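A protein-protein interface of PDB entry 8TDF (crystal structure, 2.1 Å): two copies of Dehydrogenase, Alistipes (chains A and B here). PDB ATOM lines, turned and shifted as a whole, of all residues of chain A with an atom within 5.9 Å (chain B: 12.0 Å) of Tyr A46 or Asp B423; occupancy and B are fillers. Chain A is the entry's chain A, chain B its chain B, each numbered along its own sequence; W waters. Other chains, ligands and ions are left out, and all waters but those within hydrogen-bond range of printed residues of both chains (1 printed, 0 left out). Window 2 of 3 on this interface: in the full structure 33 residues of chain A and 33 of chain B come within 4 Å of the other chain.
The side-chain amino group of Lys A45 is in salt-bridge range of the side-chain carboxylate of Asp B423 (3.5 Å).
The side-chain carboxylate (OD1) of Asp A43 is in hydrogen-bond range of the backbone NH (N) of Lys A45.
The backbone NH (N) of Tyr A46 lies within hydrogen-bond range of the side-chain carboxylate (OD1) of Asp A43 (3.1 Å).
Among the printed residues, pairs that only touch across the chains: Tyr A46 with Asp B423, Tyr A46 with Gly B424, Tyr A46 with His B425, Pro A203 with Gly B424, Trp A204 with Phe B419, Trp A204 with Gly B424, Trp A204 with Pro B426 and Trp A204 with Phe B428.
Gly A21 touches none of the printed residues of chain B.
No residue of chain B comes within 4 Å of Gly A22.
No residue of chain B comes within 4 Å of Asp A43.
Lys A45 touches just one residue of chain B: Asp B423 (3.5 Å).
Of the printed residues of chain B, Tyr A46 touches Asp B423, Gly B424 and His B425.
No residue of chain B comes within 4 Å of Asp A48.
His A49 touches none of the printed residues of chain B.
Pro A203 touches just one residue of chain B: Gly B424 (3.7 Å).
Printed residues of chain B within 4 Å of Trp A204: Phe B419 (3.9 Å), Gly B424 (3.4 Å), Pro B426 (3.5 Å) and Phe B428 (3.9 Å).
Of the printed residues of chain A, Phe B419 touches Trp A204.
Of chain A, only Lys A45 and Tyr A46 come within 4 Å of Asp B423.
Of the printed residues of chain A, Gly B424 touches Tyr A46 (3.99 Å), Pro A203 (3.7 Å) and Trp A204 (3.4 Å).
Printed residues of chain A within 4 Å of His B425: Tyr A46 (3.6 Å).
Of the printed residues of chain A, Phe B428 touches Trp A204.
The nearest printed residue of chain B that does not touch Tyr A46 is Pro B426 (5.8 Å).
Of the 10 printed residues of chain B, 6 touch a printed residue of chain A.
Hydrophobic or aromatic side chains of chain B that line the printed part of chain A: Phe B419, His B425, Pro B426 and Phe B428.
Printed residues of chain A that touch a printed residue of chain B: Lys A45, Tyr A46, Pro A203 and Trp A204.
Hydrophobic or aromatic side chains of chain A that line the printed part of chain B: Tyr A46, Pro A203 and Trp A204.
Among the printed residues, 9 pairs touch across the chains.
No position is printed for both chains.
Water W1 bridges a ring nitrogen (NE2) of His B425 (2.8 Å) and the backbone carbonyl oxygen (O) of Tyr A46 (3.0 Å).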
ATOM      1  N   GLY A  21     -21.468  -0.745  -6.482  1.00  0.00           N
ATOM      2  CA  GLY A  21     -21.706  -0.564  -5.066  1.00  0.00           C
ATOM      3  C   GLY A  21     -22.970  -1.284  -4.621  1.00  0.00           C
ATOM      4  O   GLY A  21     -23.093  -1.550  -3.444  1.00  0.00           O
ATOM      5  N   GLY A  22     -23.898  -1.566  -5.522  1.00  0.00           N
ATOM      6  CA  GLY A  22     -25.121  -2.276  -5.112  1.00  0.00           C
ATOM      7  C   GLY A  22     -25.158  -3.697  -5.712  1.00  0.00           C
ATOM      8  O   GLY A  22     -24.285  -4.492  -5.425  1.00  0.00           O
ATOM      9  N   ARG A  23     -26.022  -3.894  -6.704  1.00  0.00           N
ATOM     10  CA  ARG A  23     -26.106  -5.144  -7.402  1.00  0.00           C
ATOM     11  C   ARG A  23     -24.767  -5.545  -8.015  1.00  0.00           C
ATOM     12  O   ARG A  23     -24.464  -6.727  -8.091  1.00  0.00           O
ATOM     13  CB  ARG A  23     -27.199  -5.093  -8.464  1.00  0.00           C
ATOM     14  CG  ARG A  23     -27.262  -6.319  -9.374  1.00  0.00           C
ATOM     15  CD  ARG A  23     -27.696  -7.558  -8.558  1.00  0.00           C
ATOM     16  NE  ARG A  23     -27.801  -8.656  -9.493  1.00  0.00           N
ATOM     17  CZ  ARG A  23     -27.942  -9.928  -9.120  1.00  0.00           C
ATOM     18  NH1 ARG A  23     -27.933 -10.279  -7.856  1.00  0.00           N
ATOM     19  NH2 ARG A  23     -27.980 -10.876 -10.011  1.00  0.00           N
ATOM     20  N   ASP A  41     -16.781   3.592 -10.155  1.00  0.00           N
ATOM     21  CA  ASP A  41     -17.997   3.932  -9.450  1.00  0.00           C
ATOM     22  C   ASP A  41     -17.980   5.423  -9.175  1.00  0.00           C
ATOM     23  O   ASP A  41     -16.952   5.952  -8.815  1.00  0.00           O
ATOM     24  CB  ASP A  41     -18.248   3.148  -8.178  1.00  0.00           C
ATOM     25  CG  ASP A  41     -19.716   3.107  -7.801  1.00  0.00           C
ATOM     26  OD1 ASP A  41     -20.219   4.118  -7.348  1.00  0.00           O
ATOM     27  OD2 ASP A  41     -20.333   2.015  -7.892  1.00  0.00           O
ATOM     28  N   ASP A  43     -19.465   6.787  -6.811  1.00  0.00           N
ATOM     29  CA  ASP A  43     -19.671   7.034  -5.404  1.00  0.00           C
ATOM     30  C   ASP A  43     -18.642   6.262  -4.585  1.00  0.00           C
ATOM     31  O   ASP A  43     -18.852   5.085  -4.293  1.00  0.00           O
ATOM     32  CB  ASP A  43     -21.069   6.618  -4.964  1.00  0.00           C
ATOM     33  CG  ASP A  43     -21.493   7.030  -3.560  1.00  0.00           C
ATOM     34  OD1 ASP A  43     -20.623   7.278  -2.736  1.00  0.00           O
ATOM     35  OD2 ASP A  43     -22.781   7.186  -3.363  1.00  0.00           O
ATOM     36  N   TRP A  44     -17.599   6.945  -4.123  1.00  0.00           N
ATOM     37  CA  TRP A  44     -16.479   6.248  -3.484  1.00  0.00           C
ATOM     38  C   TRP A  44     -16.725   5.999  -2.026  1.00  0.00           C
ATOM     39  O   TRP A  44     -15.965   5.245  -1.464  1.00  0.00           O
ATOM     40  CB  TRP A  44     -15.145   6.968  -3.649  1.00  0.00           C
ATOM     41  CG  TRP A  44     -14.567   6.747  -5.014  1.00  0.00           C
ATOM     42  CD1 TRP A  44     -15.227   6.370  -6.135  1.00  0.00           C
ATOM     43  CD2 TRP A  44     -13.196   6.857  -5.361  1.00  0.00           C
ATOM     44  NE1 TRP A  44     -14.373   6.325  -7.191  1.00  0.00           N
ATOM     45  CE2 TRP A  44     -13.122   6.633  -6.760  1.00  0.00           C
ATOM     46  CE3 TRP A  44     -12.033   7.151  -4.641  1.00  0.00           C
ATOM     47  CZ2 TRP A  44     -11.900   6.665  -7.469  1.00  0.00           C
ATOM     48  CZ3 TRP A  44     -10.823   7.228  -5.360  1.00  0.00           C
ATOM     49  CH2 TRP A  44     -10.764   6.985  -6.755  1.00  0.00           C
ATOM     50  N   LYS A  45     -17.851   6.468  -1.477  1.00  0.00           N
ATOM     51  CA  LYS A  45     -18.213   6.073  -0.115  1.00  0.00           C
ATOM     52  C   LYS A  45     -19.050   4.808  -0.160  1.00  0.00           C
ATOM     53  O   LYS A  45     -18.720   3.811   0.449  1.00  0.00           O
ATOM     54  CB  LYS A  45     -18.922   7.233   0.589  1.00  0.00           C
ATOM     55  CG  LYS A  45     -19.633   6.924   1.896  1.00  0.00           C
ATOM     56  CD  LYS A  45     -19.901   8.237   2.680  1.00  0.00           C
ATOM     57  CE  LYS A  45     -20.609   8.098   4.016  1.00  0.00           C
ATOM     58  NZ  LYS A  45     -22.076   8.364   3.854  1.00  0.00           N
ATOM     59  N   TYR A  46     -20.130   4.827  -0.926  1.00  0.00           N
ATOM     60  CA  TYR A  46     -21.037   3.688  -0.971  1.00  0.00           C
ATOM     61  C   TYR A  46     -20.308   2.456  -1.513  1.00  0.00           C
ATOM     62  O   TYR A  46     -20.657   1.344  -1.180  1.00  0.00           O
ATOM     63  CB  TYR A  46     -22.166   4.082  -1.905  1.00  0.00           C
ATOM     64  CG  TYR A  46     -23.222   3.039  -2.143  1.00  0.00           C
ATOM     65  CD1 TYR A  46     -24.085   2.678  -1.132  1.00  0.00           C
ATOM     66  CD2 TYR A  46     -23.406   2.512  -3.405  1.00  0.00           C
ATOM     67  CE1 TYR A  46     -25.150   1.833  -1.394  1.00  0.00           C
ATOM     68  CE2 TYR A  46     -24.465   1.664  -3.670  1.00  0.00           C
ATOM     69  CZ  TYR A  46     -25.315   1.288  -2.648  1.00  0.00           C
ATOM     70  OH  TYR A  46     -26.360   0.488  -3.007  1.00  0.00           O
ATOM     71  N   ALA A  47     -19.377   2.662  -2.433  1.00  0.00           N
ATOM     72  CA  ALA A  47     -18.812   1.563  -3.176  1.00  0.00           C
ATOM     73  C   ALA A  47     -17.486   1.101  -2.589  1.00  0.00           C
ATOM     74  O   ALA A  47     -16.783   0.292  -3.184  1.00  0.00           O
ATOM     75  CB  ALA A  47     -18.687   1.890  -4.625  1.00  0.00           C
ATOM     76  N   ASP A  48     -17.079   1.712  -1.477  1.00  0.00           N
ATOM     77  CA  ASP A  48     -15.725   1.544  -0.971  1.00  0.00           C
ATOM     78  C   ASP A  48     -15.444   0.063  -0.632  1.00  0.00           C
ATOM     79  O   ASP A  48     -14.396  -0.474  -1.009  1.00  0.00           O
ATOM     80  CB  ASP A  48     -15.496   2.429   0.233  1.00  0.00           C
ATOM     81  CG  ASP A  48     -14.072   2.341   0.734  1.00  0.00           C
ATOM     82  OD1 ASP A  48     -13.112   2.598  -0.046  1.00  0.00           O
ATOM     83  OD2 ASP A  48     -13.918   1.922   1.888  1.00  0.00           O
ATOM     84  N   HIS A  49     -16.378  -0.585   0.074  1.00  0.00           N
ATOM     85  CA  HIS A  49     -16.249  -1.975   0.465  1.00  0.00           C
ATOM     86  C   HIS A  49     -15.990  -2.840  -0.774  1.00  0.00           C
ATOM     87  O   HIS A  49     -15.316  -3.841  -0.675  1.00  0.00           O
ATOM     88  CB  HIS A  49     -17.469  -2.442   1.303  1.00  0.00           C
ATOM     89  CG  HIS A  49     -18.673  -2.717   0.486  1.00  0.00           C
ATOM     90  ND1 HIS A  49     -19.651  -1.759   0.286  1.00  0.00           N
ATOM     91  CD2 HIS A  49     -19.096  -3.812  -0.187  1.00  0.00           C
ATOM     92  CE1 HIS A  49     -20.629  -2.257  -0.492  1.00  0.00           C
ATOM     93  NE2 HIS A  49     -20.289  -3.504  -0.817  1.00  0.00           N
ATOM     94  N   VAL A  50     -16.467  -2.438  -1.960  1.00  0.00           N
ATOM     95  CA  VAL A  50     -16.314  -3.291  -3.120  1.00  0.00           C
ATOM     96  C   VAL A  50     -14.932  -3.099  -3.700  1.00  0.00           C
ATOM     97  O   VAL A  50     -14.322  -4.085  -4.073  1.00  0.00           O
ATOM     98  CB  VAL A  50     -17.401  -3.057  -4.178  1.00  0.00           C
ATOM     99  CG1 VAL A  50     -17.246  -3.983  -5.350  1.00  0.00           C
ATOM    100  CG2 VAL A  50     -18.791  -3.179  -3.639  1.00  0.00           C
ATOM    101  N   PRO A 203     -27.491   6.894  -3.760  1.00  0.00           N
ATOM    102  CA  PRO A 203     -27.715   5.595  -4.396  1.00  0.00           C
ATOM    103  C   PRO A 203     -29.102   4.989  -4.289  1.00  0.00           C
ATOM    104  O   PRO A 203     -29.912   5.484  -3.524  1.00  0.00           O
ATOM    105  CB  PRO A 203     -26.767   4.660  -3.610  1.00  0.00           C
ATOM    106  CG  PRO A 203     -25.843   5.569  -2.804  1.00  0.00           C
ATOM    107  CD  PRO A 203     -26.632   6.851  -2.577  1.00  0.00           C
ATOM    108  N   TRP A 204     -29.383   3.984  -5.127  1.00  0.00           N
ATOM    109  CA  TRP A 204     -30.512   3.045  -5.026  1.00  0.00           C
ATOM    110  C   TRP A 204     -31.844   3.658  -5.477  1.00  0.00           C
ATOM    111  O   TRP A 204     -32.597   3.078  -6.286  1.00  0.00           O
ATOM    112  CB  TRP A 204     -30.688   2.494  -3.623  1.00  0.00           C
ATOM    113  CG  TRP A 204     -31.579   1.267  -3.601  1.00  0.00           C
ATOM    114  CD1 TRP A 204     -31.208  -0.017  -3.898  1.00  0.00           C
ATOM    115  CD2 TRP A 204     -33.022   1.253  -3.482  1.00  0.00           C
ATOM    116  NE1 TRP A 204     -32.322  -0.812  -3.929  1.00  0.00           N
ATOM    117  CE2 TRP A 204     -33.451  -0.068  -3.678  1.00  0.00           C
ATOM    118  CE3 TRP A 204     -33.982   2.233  -3.209  1.00  0.00           C
ATOM    119  CZ2 TRP A 204     -34.773  -0.472  -3.591  1.00  0.00           C
ATOM    120  CZ3 TRP A 204     -35.311   1.850  -3.163  1.00  0.00           C
ATOM    121  CH2 TRP A 204     -35.706   0.487  -3.372  1.00  0.00           C
ATOM    122  N   PHE B 419     -40.451   2.619   5.343  1.00  0.00           N
ATOM    123  CA  PHE B 419     -39.369   2.557   4.381  1.00  0.00           C
ATOM    124  C   PHE B 419     -38.371   3.623   4.750  1.00  0.00           C
ATOM    125  O   PHE B 419     -38.788   4.716   5.035  1.00  0.00           O
ATOM    126  CB  PHE B 419     -39.877   2.797   2.947  1.00  0.00           C
ATOM    127  CG  PHE B 419     -38.762   2.984   1.936  1.00  0.00           C
ATOM    128  CD1 PHE B 419     -38.171   1.912   1.346  1.00  0.00           C
ATOM    129  CD2 PHE B 419     -38.269   4.256   1.665  1.00  0.00           C
ATOM    130  CE1 PHE B 419     -37.083   2.076   0.498  1.00  0.00           C
ATOM    131  CE2 PHE B 419     -37.205   4.444   0.803  1.00  0.00           C
ATOM    132  CZ  PHE B 419     -36.594   3.347   0.219  1.00  0.00           C
ATOM    133  N   HIS B 420     -37.078   3.332   4.685  1.00  0.00           N
ATOM    134  CA  HIS B 420     -36.092   4.333   4.957  1.00  0.00           C
ATOM    135  C   HIS B 420     -34.825   3.975   4.174  1.00  0.00           C
ATOM    136  O   HIS B 420     -34.591   2.796   3.966  1.00  0.00           O
ATOM    137  CB  HIS B 420     -35.954   4.318   6.488  1.00  0.00           C
ATOM    138  CG  HIS B 420     -34.874   5.159   6.976  1.00  0.00           C
ATOM    139  ND1 HIS B 420     -33.789   4.551   7.579  1.00  0.00           N
ATOM    140  CD2 HIS B 420     -34.567   6.484   6.931  1.00  0.00           C
ATOM    141  CE1 HIS B 420     -32.875   5.486   7.972  1.00  0.00           C
ATOM    142  NE2 HIS B 420     -33.307   6.669   7.555  1.00  0.00           N
ATOM    143  N   ILE B 421     -34.025   4.968   3.781  1.00  0.00           N
ATOM    144  CA  ILE B 421     -32.722   4.782   3.169  1.00  0.00           C
ATOM    145  C   ILE B 421     -31.685   5.413   4.086  1.00  0.00           C
ATOM    146  O   ILE B 421     -31.837   6.527   4.482  1.00  0.00           O
ATOM    147  CB  ILE B 421     -32.657   5.388   1.742  1.00  0.00           C
ATOM    148  CG1 ILE B 421     -33.722   4.819   0.858  1.00  0.00           C
ATOM    149  CG2 ILE B 421     -31.335   5.129   1.067  1.00  0.00           C
ATOM    150  CD1 ILE B 421     -33.627   5.261  -0.571  1.00  0.00           C
ATOM    151  N   LYS B 422     -30.609   4.709   4.369  1.00  0.00           N
ATOM    152  CA  LYS B 422     -29.492   5.137   5.164  1.00  0.00           C
ATOM    153  C   LYS B 422     -28.215   5.001   4.354  1.00  0.00           C
ATOM    154  O   LYS B 422     -27.804   3.877   4.136  1.00  0.00           O
ATOM    155  CB  LYS B 422     -29.305   4.100   6.284  1.00  0.00           C
ATOM    156  CG  LYS B 422     -29.987   4.423   7.591  1.00  0.00           C
ATOM    157  CD  LYS B 422     -29.022   4.591   8.736  1.00  0.00           C
ATOM    158  CE  LYS B 422     -27.840   5.464   8.386  1.00  0.00           C
ATOM    159  NZ  LYS B 422     -26.678   4.956   9.140  1.00  0.00           N
ATOM    160  N   ASP B 423     -27.594   6.115   3.922  1.00  0.00           N
ATOM    161  CA  ASP B 423     -26.319   6.066   3.197  1.00  0.00           C
ATOM    162  C   ASP B 423     -26.472   5.196   1.930  1.00  0.00           C
ATOM    163  O   ASP B 423     -25.640   4.380   1.590  1.00  0.00           O
ATOM    164  CB  ASP B 423     -25.169   5.605   4.112  1.00  0.00           C
ATOM    165  CG  ASP B 423     -24.816   6.507   5.302  1.00  0.00           C
ATOM    166  OD1 ASP B 423     -25.504   7.516   5.547  1.00  0.00           O
ATOM    167  OD2 ASP B 423     -23.805   6.224   5.983  1.00  0.00           O
ATOM    168  N   GLY B 424     -27.594   5.328   1.246  1.00  0.00           N
ATOM    169  CA  GLY B 424     -27.886   4.487   0.092  1.00  0.00           C
ATOM    170  C   GLY B 424     -28.529   3.107   0.307  1.00  0.00           C
ATOM    171  O   GLY B 424     -29.044   2.607  -0.663  1.00  0.00           O
ATOM    172  N   HIS B 425     -28.539   2.566   1.519  1.00  0.00           N
ATOM    173  CA  HIS B 425     -29.054   1.225   1.773  1.00  0.00           C
ATOM    174  C   HIS B 425     -30.510   1.260   2.175  1.00  0.00           C
ATOM    175  O   HIS B 425     -30.866   1.847   3.179  1.00  0.00           O
ATOM    176  CB  HIS B 425     -28.234   0.589   2.892  1.00  0.00           C
ATOM    177  CG  HIS B 425     -26.840   0.397   2.440  1.00  0.00           C
ATOM    178  ND1 HIS B 425     -26.529  -0.647   1.600  1.00  0.00           N
ATOM    179  CD2 HIS B 425     -25.714   1.114   2.592  1.00  0.00           C
ATOM    180  CE1 HIS B 425     -25.212  -0.612   1.320  1.00  0.00           C
ATOM    181  NE2 HIS B 425     -24.681   0.437   1.923  1.00  0.00           N
ATOM    182  N   PRO B 426     -31.429   0.693   1.389  1.00  0.00           N
ATOM    183  CA  PRO B 426     -32.829   0.711   1.734  1.00  0.00           C
ATOM    184  C   PRO B 426     -33.164  -0.336   2.810  1.00  0.00           C
ATOM    185  O   PRO B 426     -32.543  -1.325   2.892  1.00  0.00           O
ATOM    186  CB  PRO B 426     -33.474   0.399   0.371  1.00  0.00           C
ATOM    187  CG  PRO B 426     -32.509  -0.513  -0.288  1.00  0.00           C
ATOM    188  CD  PRO B 426     -31.161  -0.031   0.155  1.00  0.00           C
ATOM    189  N   THR B 427     -34.128  -0.020   3.635  1.00  0.00           N
ATOM    190  CA  THR B 427     -34.744  -0.834   4.659  1.00  0.00           C
ATOM    191  C   THR B 427     -36.210  -0.835   4.400  1.00  0.00           C
ATOM    192  O   THR B 427     -36.774   0.268   4.287  1.00  0.00           O
ATOM    193  CB  THR B 427     -34.603  -0.170   6.032  1.00  0.00           C
ATOM    194  OG1 THR B 427     -33.222  -0.292   6.303  1.00  0.00           O
ATOM    195  CG2 THR B 427     -35.351  -0.863   7.129  1.00  0.00           C
ATOM    196  N   PHE B 428     -36.840  -1.991   4.501  1.00  0.00           N
ATOM    197  CA  PHE B 428     -38.246  -2.108   4.173  1.00  0.00           C
ATOM    198  C   PHE B 428     -39.151  -2.410   5.349  1.00  0.00           C
ATOM    199  O   PHE B 428     -40.049  -3.223   5.206  1.00  0.00           O
ATOM    200  CB  PHE B 428     -38.448  -3.196   3.133  1.00  0.00           C
ATOM    201  CG  PHE B 428     -37.763  -2.829   1.848  1.00  0.00           C
ATOM    202  CD1 PHE B 428     -38.368  -1.943   0.980  1.00  0.00           C
ATOM    203  CD2 PHE B 428     -36.448  -3.260   1.597  1.00  0.00           C
ATOM    204  CE1 PHE B 428     -37.703  -1.580  -0.163  1.00  0.00           C
ATOM    205  CE2 PHE B 428     -35.792  -2.846   0.455  1.00  0.00           C
ATOM    206  CZ  PHE B 428     -36.419  -2.009  -0.413  1.00  0.00           C
HETATM  207  O   HOH W   1     -22.037   1.091   1.436  1.00  0.00           O
